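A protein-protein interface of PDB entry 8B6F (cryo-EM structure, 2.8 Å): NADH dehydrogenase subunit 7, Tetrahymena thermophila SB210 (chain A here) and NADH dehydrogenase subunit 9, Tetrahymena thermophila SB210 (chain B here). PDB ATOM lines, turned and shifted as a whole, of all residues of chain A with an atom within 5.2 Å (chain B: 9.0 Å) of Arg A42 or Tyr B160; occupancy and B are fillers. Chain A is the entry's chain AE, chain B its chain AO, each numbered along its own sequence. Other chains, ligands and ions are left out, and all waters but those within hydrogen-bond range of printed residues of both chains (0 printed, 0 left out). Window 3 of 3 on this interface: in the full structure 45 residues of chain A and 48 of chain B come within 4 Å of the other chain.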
ATOM      1  N   ASN A  29      20.067  -9.215  37.817  1.00  0.00           N
ATOM      2  CA  ASN A  29      20.987  -8.707  36.800  1.00  0.00           C
ATOM      3  C   ASN A  29      22.050  -7.873  37.506  1.00  0.00           C
ATOM      4  O   ASN A  29      21.992  -6.645  37.552  1.00  0.00           O
ATOM      5  CB  ASN A  29      20.244  -7.891  35.748  1.00  0.00           C
ATOM      6  CG  ASN A  29      19.412  -8.749  34.821  1.00  0.00           C
ATOM      7  OD1 ASN A  29      19.854  -9.109  33.731  1.00  0.00           O
ATOM      8  ND2 ASN A  29      18.201  -9.083  35.248  1.00  0.00           N
ATOM      9  N   PHE A  30      23.034  -8.564  38.074  1.00  0.00           N
ATOM     10  CA  PHE A  30      24.164  -7.883  38.692  1.00  0.00           C
ATOM     11  C   PHE A  30      24.888  -7.068  37.629  1.00  0.00           C
ATOM     12  O   PHE A  30      25.513  -7.630  36.726  1.00  0.00           O
ATOM     13  CB  PHE A  30      25.096  -8.908  39.342  1.00  0.00           C
ATOM     14  CG  PHE A  30      26.269  -8.304  40.055  1.00  0.00           C
ATOM     15  CD1 PHE A  30      26.167  -7.919  41.381  1.00  0.00           C
ATOM     16  CD2 PHE A  30      27.481  -8.144  39.405  1.00  0.00           C
ATOM     17  CE1 PHE A  30      27.250  -7.371  42.042  1.00  0.00           C
ATOM     18  CE2 PHE A  30      28.569  -7.597  40.060  1.00  0.00           C
ATOM     19  CZ  PHE A  30      28.453  -7.211  41.380  1.00  0.00           C
ATOM     20  N   GLY A  31      24.817  -5.744  37.734  1.00  0.00           N
ATOM     21  CA  GLY A  31      25.329  -4.875  36.704  1.00  0.00           C
ATOM     22  C   GLY A  31      24.373  -4.775  35.533  1.00  0.00           C
ATOM     23  O   GLY A  31      23.266  -5.322  35.559  1.00  0.00           O
ATOM     24  N   PRO A  32      24.781  -4.067  34.474  1.00  0.00           N
ATOM     25  CA  PRO A  32      26.054  -3.343  34.330  1.00  0.00           C
ATOM     26  C   PRO A  32      26.139  -2.119  35.226  1.00  0.00           C
ATOM     27  O   PRO A  32      27.202  -1.798  35.745  1.00  0.00           O
ATOM     28  CB  PRO A  32      26.060  -2.950  32.846  1.00  0.00           C
ATOM     29  CG  PRO A  32      24.616  -2.905  32.455  1.00  0.00           C
ATOM     30  CD  PRO A  32      23.961  -3.991  33.254  1.00  0.00           C
ATOM     31  N   VAL A  40      30.376  -2.787  32.851  1.00  0.00           N
ATOM     32  CA  VAL A  40      30.005  -3.404  31.584  1.00  0.00           C
ATOM     33  C   VAL A  40      29.832  -4.905  31.761  1.00  0.00           C
ATOM     34  O   VAL A  40      29.950  -5.670  30.798  1.00  0.00           O
ATOM     35  CB  VAL A  40      31.050  -3.092  30.500  1.00  0.00           C
ATOM     36  CG1 VAL A  40      31.033  -1.614  30.179  1.00  0.00           C
ATOM     37  CG2 VAL A  40      32.435  -3.525  30.954  1.00  0.00           C
ATOM     38  N   LEU A  41      29.551  -5.338  32.985  1.00  0.00           N
ATOM     39  CA  LEU A  41      29.312  -6.743  33.283  1.00  0.00           C
ATOM     40  C   LEU A  41      27.833  -6.928  33.581  1.00  0.00           C
ATOM     41  O   LEU A  41      27.300  -6.294  34.497  1.00  0.00           O
ATOM     42  CB  LEU A  41      30.155  -7.203  34.471  1.00  0.00           C
ATOM     43  CG  LEU A  41      29.961  -8.657  34.914  1.00  0.00           C
ATOM     44  CD1 LEU A  41      30.383  -9.620  33.817  1.00  0.00           C
ATOM     45  CD2 LEU A  41      30.720  -8.943  36.199  1.00  0.00           C
ATOM     46  N   ARG A  42      27.176  -7.788  32.814  1.00  0.00           N
ATOM     47  CA  ARG A  42      25.783  -8.143  33.054  1.00  0.00           C
ATOM     48  C   ARG A  42      25.779  -9.598  33.506  1.00  0.00           C
ATOM     49  O   ARG A  42      25.674 -10.517  32.695  1.00  0.00           O
ATOM     50  CB  ARG A  42      24.934  -7.935  31.808  1.00  0.00           C
ATOM     51  CG  ARG A  42      23.459  -8.207  32.027  1.00  0.00           C
ATOM     52  CD  ARG A  42      22.657  -7.970  30.762  1.00  0.00           C
ATOM     53  NE  ARG A  42      21.248  -8.285  30.955  1.00  0.00           N
ATOM     54  CZ  ARG A  42      20.321  -8.183  30.015  1.00  0.00           C
ATOM     55  NH1 ARG A  42      20.617  -7.776  28.792  1.00  0.00           N
ATOM     56  NH2 ARG A  42      19.063  -8.495  30.309  1.00  0.00           N
ATOM     57  N   LEU A  43      25.910  -9.798  34.813  1.00  0.00           N
ATOM     58  CA  LEU A  43      25.973 -11.133  35.394  1.00  0.00           C
ATOM     59  C   LEU A  43      24.570 -11.523  35.837  1.00  0.00           C
ATOM     60  O   LEU A  43      24.010 -10.909  36.751  1.00  0.00           O
ATOM     61  CB  LEU A  43      26.959 -11.157  36.559  1.00  0.00           C
ATOM     62  CG  LEU A  43      27.105 -12.472  37.326  1.00  0.00           C
ATOM     63  CD1 LEU A  43      27.759 -13.530  36.459  1.00  0.00           C
ATOM     64  CD2 LEU A  43      27.903 -12.256  38.597  1.00  0.00           C
ATOM     65  N   ILE A  44      23.997 -12.536  35.196  1.00  0.00           N
ATOM     66  CA  ILE A  44      22.736 -13.107  35.656  1.00  0.00           C
ATOM     67  C   ILE A  44      23.062 -14.029  36.823  1.00  0.00           C
ATOM     68  O   ILE A  44      23.683 -15.079  36.643  1.00  0.00           O
ATOM     69  CB  ILE A  44      22.002 -13.854  34.538  1.00  0.00           C
ATOM     70  CG1 ILE A  44      22.055 -13.060  33.229  1.00  0.00           C
ATOM     71  CG2 ILE A  44      20.558 -14.109  34.937  1.00  0.00           C
ATOM     72  CD1 ILE A  44      21.576 -11.625  33.351  1.00  0.00           C
ATOM     73  N   ASP A  56      25.675 -16.600  35.013  1.00  0.00           N
ATOM     74  CA  ASP A  56      25.629 -16.455  33.559  1.00  0.00           C
ATOM     75  C   ASP A  56      26.161 -15.067  33.232  1.00  0.00           C
ATOM     76  O   ASP A  56      25.389 -14.105  33.123  1.00  0.00           O
ATOM     77  CB  ASP A  56      24.216 -16.656  33.022  1.00  0.00           C
ATOM     78  CG  ASP A  56      24.180 -16.803  31.515  1.00  0.00           C
ATOM     79  OD1 ASP A  56      25.112 -16.316  30.845  1.00  0.00           O
ATOM     80  OD2 ASP A  56      23.212 -17.400  30.999  1.00  0.00           O
ATOM     81  N   PRO A  57      27.473 -14.923  33.069  1.00  0.00           N
ATOM     82  CA  PRO A  57      28.033 -13.605  32.751  1.00  0.00           C
ATOM     83  C   PRO A  57      27.876 -13.257  31.280  1.00  0.00           C
ATOM     84  O   PRO A  57      28.093 -14.087  30.394  1.00  0.00           O
ATOM     85  CB  PRO A  57      29.515 -13.739  33.135  1.00  0.00           C
ATOM     86  CG  PRO A  57      29.630 -15.038  33.879  1.00  0.00           C
ATOM     87  CD  PRO A  57      28.528 -15.899  33.380  1.00  0.00           C
ATOM     88  N   HIS A  58      27.489 -12.009  31.029  1.00  0.00           N
ATOM     89  CA  HIS A  58      27.538 -11.414  29.701  1.00  0.00           C
ATOM     90  C   HIS A  58      28.548 -10.279  29.748  1.00  0.00           C
ATOM     91  O   HIS A  58      28.423  -9.367  30.572  1.00  0.00           O
ATOM     92  CB  HIS A  58      26.165 -10.898  29.262  1.00  0.00           C
ATOM     93  CG  HIS A  58      25.059 -11.891  29.437  1.00  0.00           C
ATOM     94  ND1 HIS A  58      24.955 -13.033  28.674  1.00  0.00           N
ATOM     95  CD2 HIS A  58      24.000 -11.905  30.279  1.00  0.00           C
ATOM     96  CE1 HIS A  58      23.885 -13.712  29.044  1.00  0.00           C
ATOM     97  NE2 HIS A  58      23.287 -13.049  30.016  1.00  0.00           N
ATOM     98  N   LEU A  61      29.207  -6.016  26.679  1.00  0.00           N
ATOM     99  CA  LEU A  61      28.788  -4.626  26.789  1.00  0.00           C
ATOM    100  C   LEU A  61      29.922  -3.647  26.518  1.00  0.00           C
ATOM    101  O   LEU A  61      29.661  -2.444  26.410  1.00  0.00           O
ATOM    102  CB  LEU A  61      28.197  -4.365  28.175  1.00  0.00           C
ATOM    103  CG  LEU A  61      27.025  -5.264  28.583  1.00  0.00           C
ATOM    104  CD1 LEU A  61      26.497  -4.857  29.943  1.00  0.00           C
ATOM    105  CD2 LEU A  61      25.911  -5.230  27.553  1.00  0.00           C
ATOM    106  N   TRP B 134      35.293 -20.210  27.224  1.00  0.00           N
ATOM    107  CA  TRP B 134      35.068 -18.880  26.666  1.00  0.00           C
ATOM    108  C   TRP B 134      35.966 -18.609  25.468  1.00  0.00           C
ATOM    109  O   TRP B 134      35.560 -17.899  24.542  1.00  0.00           O
ATOM    110  CB  TRP B 134      35.279 -17.810  27.734  1.00  0.00           C
ATOM    111  CG  TRP B 134      34.220 -17.798  28.790  1.00  0.00           C
ATOM    112  CD1 TRP B 134      33.271 -18.754  29.013  1.00  0.00           C
ATOM    113  CD2 TRP B 134      33.998 -16.778  29.769  1.00  0.00           C
ATOM    114  NE1 TRP B 134      32.477 -18.392  30.072  1.00  0.00           N
ATOM    115  CE2 TRP B 134      32.903 -17.184  30.555  1.00  0.00           C
ATOM    116  CE3 TRP B 134      34.624 -15.562  30.062  1.00  0.00           C
ATOM    117  CZ2 TRP B 134      32.417 -16.416  31.609  1.00  0.00           C
ATOM    118  CZ3 TRP B 134      34.141 -14.801  31.109  1.00  0.00           C
ATOM    119  CH2 TRP B 134      33.047 -15.231  31.871  1.00  0.00           C
ATOM    120  N   ARG B 154      26.784 -20.761  23.546  1.00  0.00           N
ATOM    121  CA  ARG B 154      26.186 -19.436  23.520  1.00  0.00           C
ATOM    122  C   ARG B 154      27.248 -18.370  23.267  1.00  0.00           C
ATOM    123  O   ARG B 154      28.410 -18.513  23.652  1.00  0.00           O
ATOM    124  CB  ARG B 154      25.451 -19.166  24.832  1.00  0.00           C
ATOM    125  CG  ARG B 154      24.121 -19.902  24.932  1.00  0.00           C
ATOM    126  CD  ARG B 154      23.604 -19.996  26.359  1.00  0.00           C
ATOM    127  NE  ARG B 154      23.728 -18.736  27.083  1.00  0.00           N
ATOM    128  CZ  ARG B 154      24.661 -18.467  27.985  1.00  0.00           C
ATOM    129  NH1 ARG B 154      25.578 -19.360  28.327  1.00  0.00           N
ATOM    130  NH2 ARG B 154      24.680 -17.268  28.560  1.00  0.00           N
ATOM    131  N   LYS B 155      26.835 -17.294  22.604  1.00  0.00           N
ATOM    132  CA  LYS B 155      27.765 -16.253  22.199  1.00  0.00           C
ATOM    133  C   LYS B 155      28.361 -15.548  23.413  1.00  0.00           C
ATOM    134  O   LYS B 155      27.780 -15.515  24.501  1.00  0.00           O
ATOM    135  CB  LYS B 155      27.075 -15.223  21.304  1.00  0.00           C
ATOM    136  CG  LYS B 155      26.634 -15.765  19.955  1.00  0.00           C
ATOM    137  CD  LYS B 155      26.030 -14.676  19.079  1.00  0.00           C
ATOM    138  CE  LYS B 155      24.741 -14.119  19.671  1.00  0.00           C
ATOM    139  NZ  LYS B 155      24.113 -13.103  18.779  1.00  0.00           N
ATOM    140  N   LEU B 156      29.542 -14.975  23.204  1.00  0.00           N
ATOM    141  CA  LEU B 156      30.259 -14.251  24.246  1.00  0.00           C
ATOM    142  C   LEU B 156      31.017 -13.116  23.580  1.00  0.00           C
ATOM    143  O   LEU B 156      31.932 -13.374  22.796  1.00  0.00           O
ATOM    144  CB  LEU B 156      31.219 -15.180  24.992  1.00  0.00           C
ATOM    145  CG  LEU B 156      31.916 -14.614  26.227  1.00  0.00           C
ATOM    146  CD1 LEU B 156      30.950 -14.540  27.399  1.00  0.00           C
ATOM    147  CD2 LEU B 156      33.128 -15.448  26.580  1.00  0.00           C
ATOM    148  N   LEU B 157      30.675 -11.876  23.929  1.00  0.00           N
ATOM    149  CA  LEU B 157      31.177 -10.640  23.319  1.00  0.00           C
ATOM    150  C   LEU B 157      30.451 -10.231  22.043  1.00  0.00           C
ATOM    151  O   LEU B 157      30.932  -9.322  21.353  1.00  0.00           O
ATOM    152  CB  LEU B 157      32.672 -10.713  22.982  1.00  0.00           C
ATOM    153  CG  LEU B 157      33.622 -11.113  24.108  1.00  0.00           C
ATOM    154  CD1 LEU B 157      35.015 -11.355  23.559  1.00  0.00           C
ATOM    155  CD2 LEU B 157      33.650 -10.039  25.177  1.00  0.00           C
ATOM    156  N   LEU B 158      29.324 -10.847  21.697  1.00  0.00           N
ATOM    157  CA  LEU B 158      28.523 -10.410  20.562  1.00  0.00           C
ATOM    158  C   LEU B 158      27.168  -9.898  21.033  1.00  0.00           C
ATOM    159  O   LEU B 158      26.665 -10.290  22.089  1.00  0.00           O
ATOM    160  CB  LEU B 158      28.322 -11.529  19.535  1.00  0.00           C
ATOM    161  CG  LEU B 158      29.347 -11.635  18.397  1.00  0.00           C
ATOM    162  CD1 LEU B 158      28.922 -12.723  17.432  1.00  0.00           C
ATOM    163  CD2 LEU B 158      29.544 -10.326  17.643  1.00  0.00           C
ATOM    164  N   ASP B 159      26.581  -9.017  20.227  1.00  0.00           N
ATOM    165  CA  ASP B 159      25.336  -8.358  20.585  1.00  0.00           C
ATOM    166  C   ASP B 159      24.171  -9.346  20.567  1.00  0.00           C
ATOM    167  O   ASP B 159      24.237 -10.421  19.965  1.00  0.00           O
ATOM    168  CB  ASP B 159      25.061  -7.204  19.622  1.00  0.00           C
ATOM    169  CG  ASP B 159      23.932  -6.314  20.085  1.00  0.00           C
ATOM    170  OD1 ASP B 159      23.380  -6.571  21.174  1.00  0.00           O
ATOM    171  OD2 ASP B 159      23.596  -5.355  19.359  1.00  0.00           O
ATOM    172  N   TYR B 160      23.093  -8.966  21.248  1.00  0.00           N
ATOM    173  CA  TYR B 160      21.908  -9.808  21.314  1.00  0.00           C
ATOM    174  C   TYR B 160      21.153  -9.801  19.990  1.00  0.00           C
ATOM    175  O   TYR B 160      21.118  -8.798  19.272  1.00  0.00           O
ATOM    176  CB  TYR B 160      20.975  -9.332  22.427  1.00  0.00           C
ATOM    177  CG  TYR B 160      21.601  -9.308  23.799  1.00  0.00           C
ATOM    178  CD1 TYR B 160      21.931 -10.486  24.453  1.00  0.00           C
ATOM    179  CD2 TYR B 160      21.832  -8.107  24.453  1.00  0.00           C
ATOM    180  CE1 TYR B 160      22.494 -10.468  25.713  1.00  0.00           C
ATOM    181  CE2 TYR B 160      22.395  -8.078  25.712  1.00  0.00           C
ATOM    182  CZ  TYR B 160      22.723  -9.261  26.337  1.00  0.00           C
ATOM    183  OH  TYR B 160      23.280  -9.233  27.593  1.00  0.00           O
ATOM    184  N   SER B 161      20.531 -10.937  19.680  1.00  0.00           N
ATOM    185  CA  SER B 161      19.663 -11.065  18.510  1.00  0.00           C
ATOM    186  C   SER B 161      20.379 -10.623  17.237  1.00  0.00           C
ATOM    187  O   SER B 161      19.818  -9.922  16.393  1.00  0.00           O
ATOM    188  CB  SER B 161      18.366 -10.282  18.707  1.00  0.00           C
ATOM    189  OG  SER B 161      18.623  -8.909  18.924  1.00  0.00           O
ATOM    190  N   LYS B 162      21.636 -11.039  17.100  1.00  0.00           N
ATOM    191  CA  LYS B 162      22.416 -10.769  15.904  1.00  0.00           C
ATOM    192  C   LYS B 162      23.284 -11.979  15.596  1.00  0.00           C
ATOM    193  O   LYS B 162      23.814 -12.619  16.507  1.00  0.00           O
ATOM    194  CB  LYS B 162      23.296  -9.524  16.067  1.00  0.00           C
ATOM    195  CG  LYS B 162      23.943  -9.063  14.768  1.00  0.00           C
ATOM    196  CD  LYS B 162      25.037  -8.035  15.005  1.00  0.00           C
ATOM    197  CE  LYS B 162      24.503  -6.790  15.686  1.00  0.00           C
ATOM    198  NZ  LYS B 162      25.536  -5.717  15.763  1.00  0.00           N
ATOM    199  N   ILE B 163      23.418 -12.287  14.310  1.00  0.00           N
ATOM    200  CA  ILE B 163      24.241 -13.393  13.835  1.00  0.00           C
ATOM    201  C   ILE B 163      25.256 -12.822  12.858  1.00  0.00           C
ATOM    202  O   ILE B 163      24.878 -12.221  11.845  1.00  0.00           O
ATOM    203  CB  ILE B 163      23.397 -14.490  13.171  1.00  0.00           C
ATOM    204  CG1 ILE B 163      22.356 -15.026  14.159  1.00  0.00           C
ATOM    205  CG2 ILE B 163      24.297 -15.608  12.656  1.00  0.00           C
ATOM    206  CD1 ILE B 163      21.358 -15.982  13.544  1.00  0.00           C
ATOM    207  N   GLU B 164      26.538 -13.007  13.158  1.00  0.00           N
ATOM    208  CA  GLU B 164      27.598 -12.504  12.296  1.00  0.00           C
ATOM    209  C   GLU B 164      28.930 -13.047  12.788  1.00  0.00           C
ATOM    210  O   GLU B 164      29.050 -13.517  13.922  1.00  0.00           O
ATOM    211  CB  GLU B 164      27.621 -10.974  12.267  1.00  0.00           C
ATOM    212  CG  GLU B 164      27.787 -10.339  13.636  1.00  0.00           C
ATOM    213  CD  GLU B 164      27.862  -8.829  13.570  1.00  0.00           C
ATOM    214  OE1 GLU B 164      27.651  -8.274  12.473  1.00  0.00           O
ATOM    215  OE2 GLU B 164      28.134  -8.198  14.613  1.00  0.00           O
ATOM    216  N   GLN B 177      24.855  -2.627  10.184  1.00  0.00           N
ATOM    217  CA  GLN B 177      23.687  -1.937  10.709  1.00  0.00           C
ATOM    218  C   GLN B 177      24.100  -1.088  11.901  1.00  0.00           C
ATOM    219  O   GLN B 177      25.071  -1.397  12.596  1.00  0.00           O
ATOM    220  CB  GLN B 177      22.587  -2.928  11.109  1.00  0.00           C
ATOM    221  CG  GLN B 177      22.997  -3.906  12.195  1.00  0.00           C
ATOM    222  CD  GLN B 177      21.987  -5.017  12.383  1.00  0.00           C
ATOM    223  OE1 GLN B 177      21.289  -5.400  11.448  1.00  0.00           O
ATOM    224  NE2 GLN B 177      21.910  -5.547  13.596  1.00  0.00           N
ATOM    225  N   VAL B 190      17.400  -0.884  15.459  1.00  0.00           N
ATOM    226  CA  VAL B 190      18.567  -1.115  14.617  1.00  0.00           C
ATOM    227  C   VAL B 190      18.120  -1.049  13.165  1.00  0.00           C
ATOM    228  O   VAL B 190      17.101  -1.642  12.797  1.00  0.00           O
ATOM    229  CB  VAL B 190      19.236  -2.468  14.930  1.00  0.00           C
ATOM    230  CG1 VAL B 190      18.330  -3.636  14.548  1.00  0.00           C
ATOM    231  CG2 VAL B 190      20.572  -2.572  14.228  1.00  0.00           C
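Of the 13 printed residues of chain A, 4 touch a printed residue of chain B. Printed residues of chain A that touch a printed residue of chain B: Arg A42, Asp A56, Pro A57 and His A58. Hydrophobic or aromatic side chains of chain A that line the printed part of chain B: Pro A57 and His A58. Hydrophobic or aromatic side chains of chain B that line the printed part of chain A: Trp B134 and Tyr B160. Among the printed residues, 5 pairs touch across the chains. Among the printed residues, Asp or Glu carboxylates within 4 Å of a Lys or Arg side-chain nitrogen of the other chain: Asp A56 with Arg B154 (2.5 Å).
The backbone carbonyl oxygen (O) of Asp A56 sits at hydrogen-bond distance from the backbone NH (N) of Ile A44 (2.9 Å). The side-chain amide oxygen of Asn A29 lies within hydrogen-bond range of the guanidinium group of Arg A42 (3.2 Å). The backbone carbonyl oxygen (O) of Arg A42 is in hydrogen-bond range of the backbone NH (N) of His A58 (2.9 Å).
The side-chain carboxylate of Asp A56 is in salt-bridge range of the guanidinium group of Arg B154, at 2.5 Å. The guanidinium group (NH1) of Arg A42 lies within hydrogen-bond range of the side-chain hydroxyl (OH) of Tyr B160, 3.3 Å away.
Pro A57 touches Trp B134. Arg B154 touches His A58. His A58 touches Tyr B160.
Arg A42 touches one residue of chain B. Tyr B160 touches just these residues of chain A: Arg A42 and His A58. Of chain B, only Arg B154 and Tyr B160 come within 4 Å of His A58. Of the printed residues of chain A, Trp B134 touches Pro A57 (3.8 Å). Printed residues of chain B within 4 Å of Pro A57: Trp B134. Of the printed residues of chain A, Arg B154 touches Asp A56 (2.5 Å) and His A58 (3.7 Å). Leu B157 touches none of the printed residues of chain A. Asn A29 touches none of the printed residues of chain B. The nearest residue of chain B that does not touch Arg A42 is Arg B154 (8.0 Å). The nearest residue of chain A that does not touch Tyr B160 is Leu A61 (4.8 Å).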
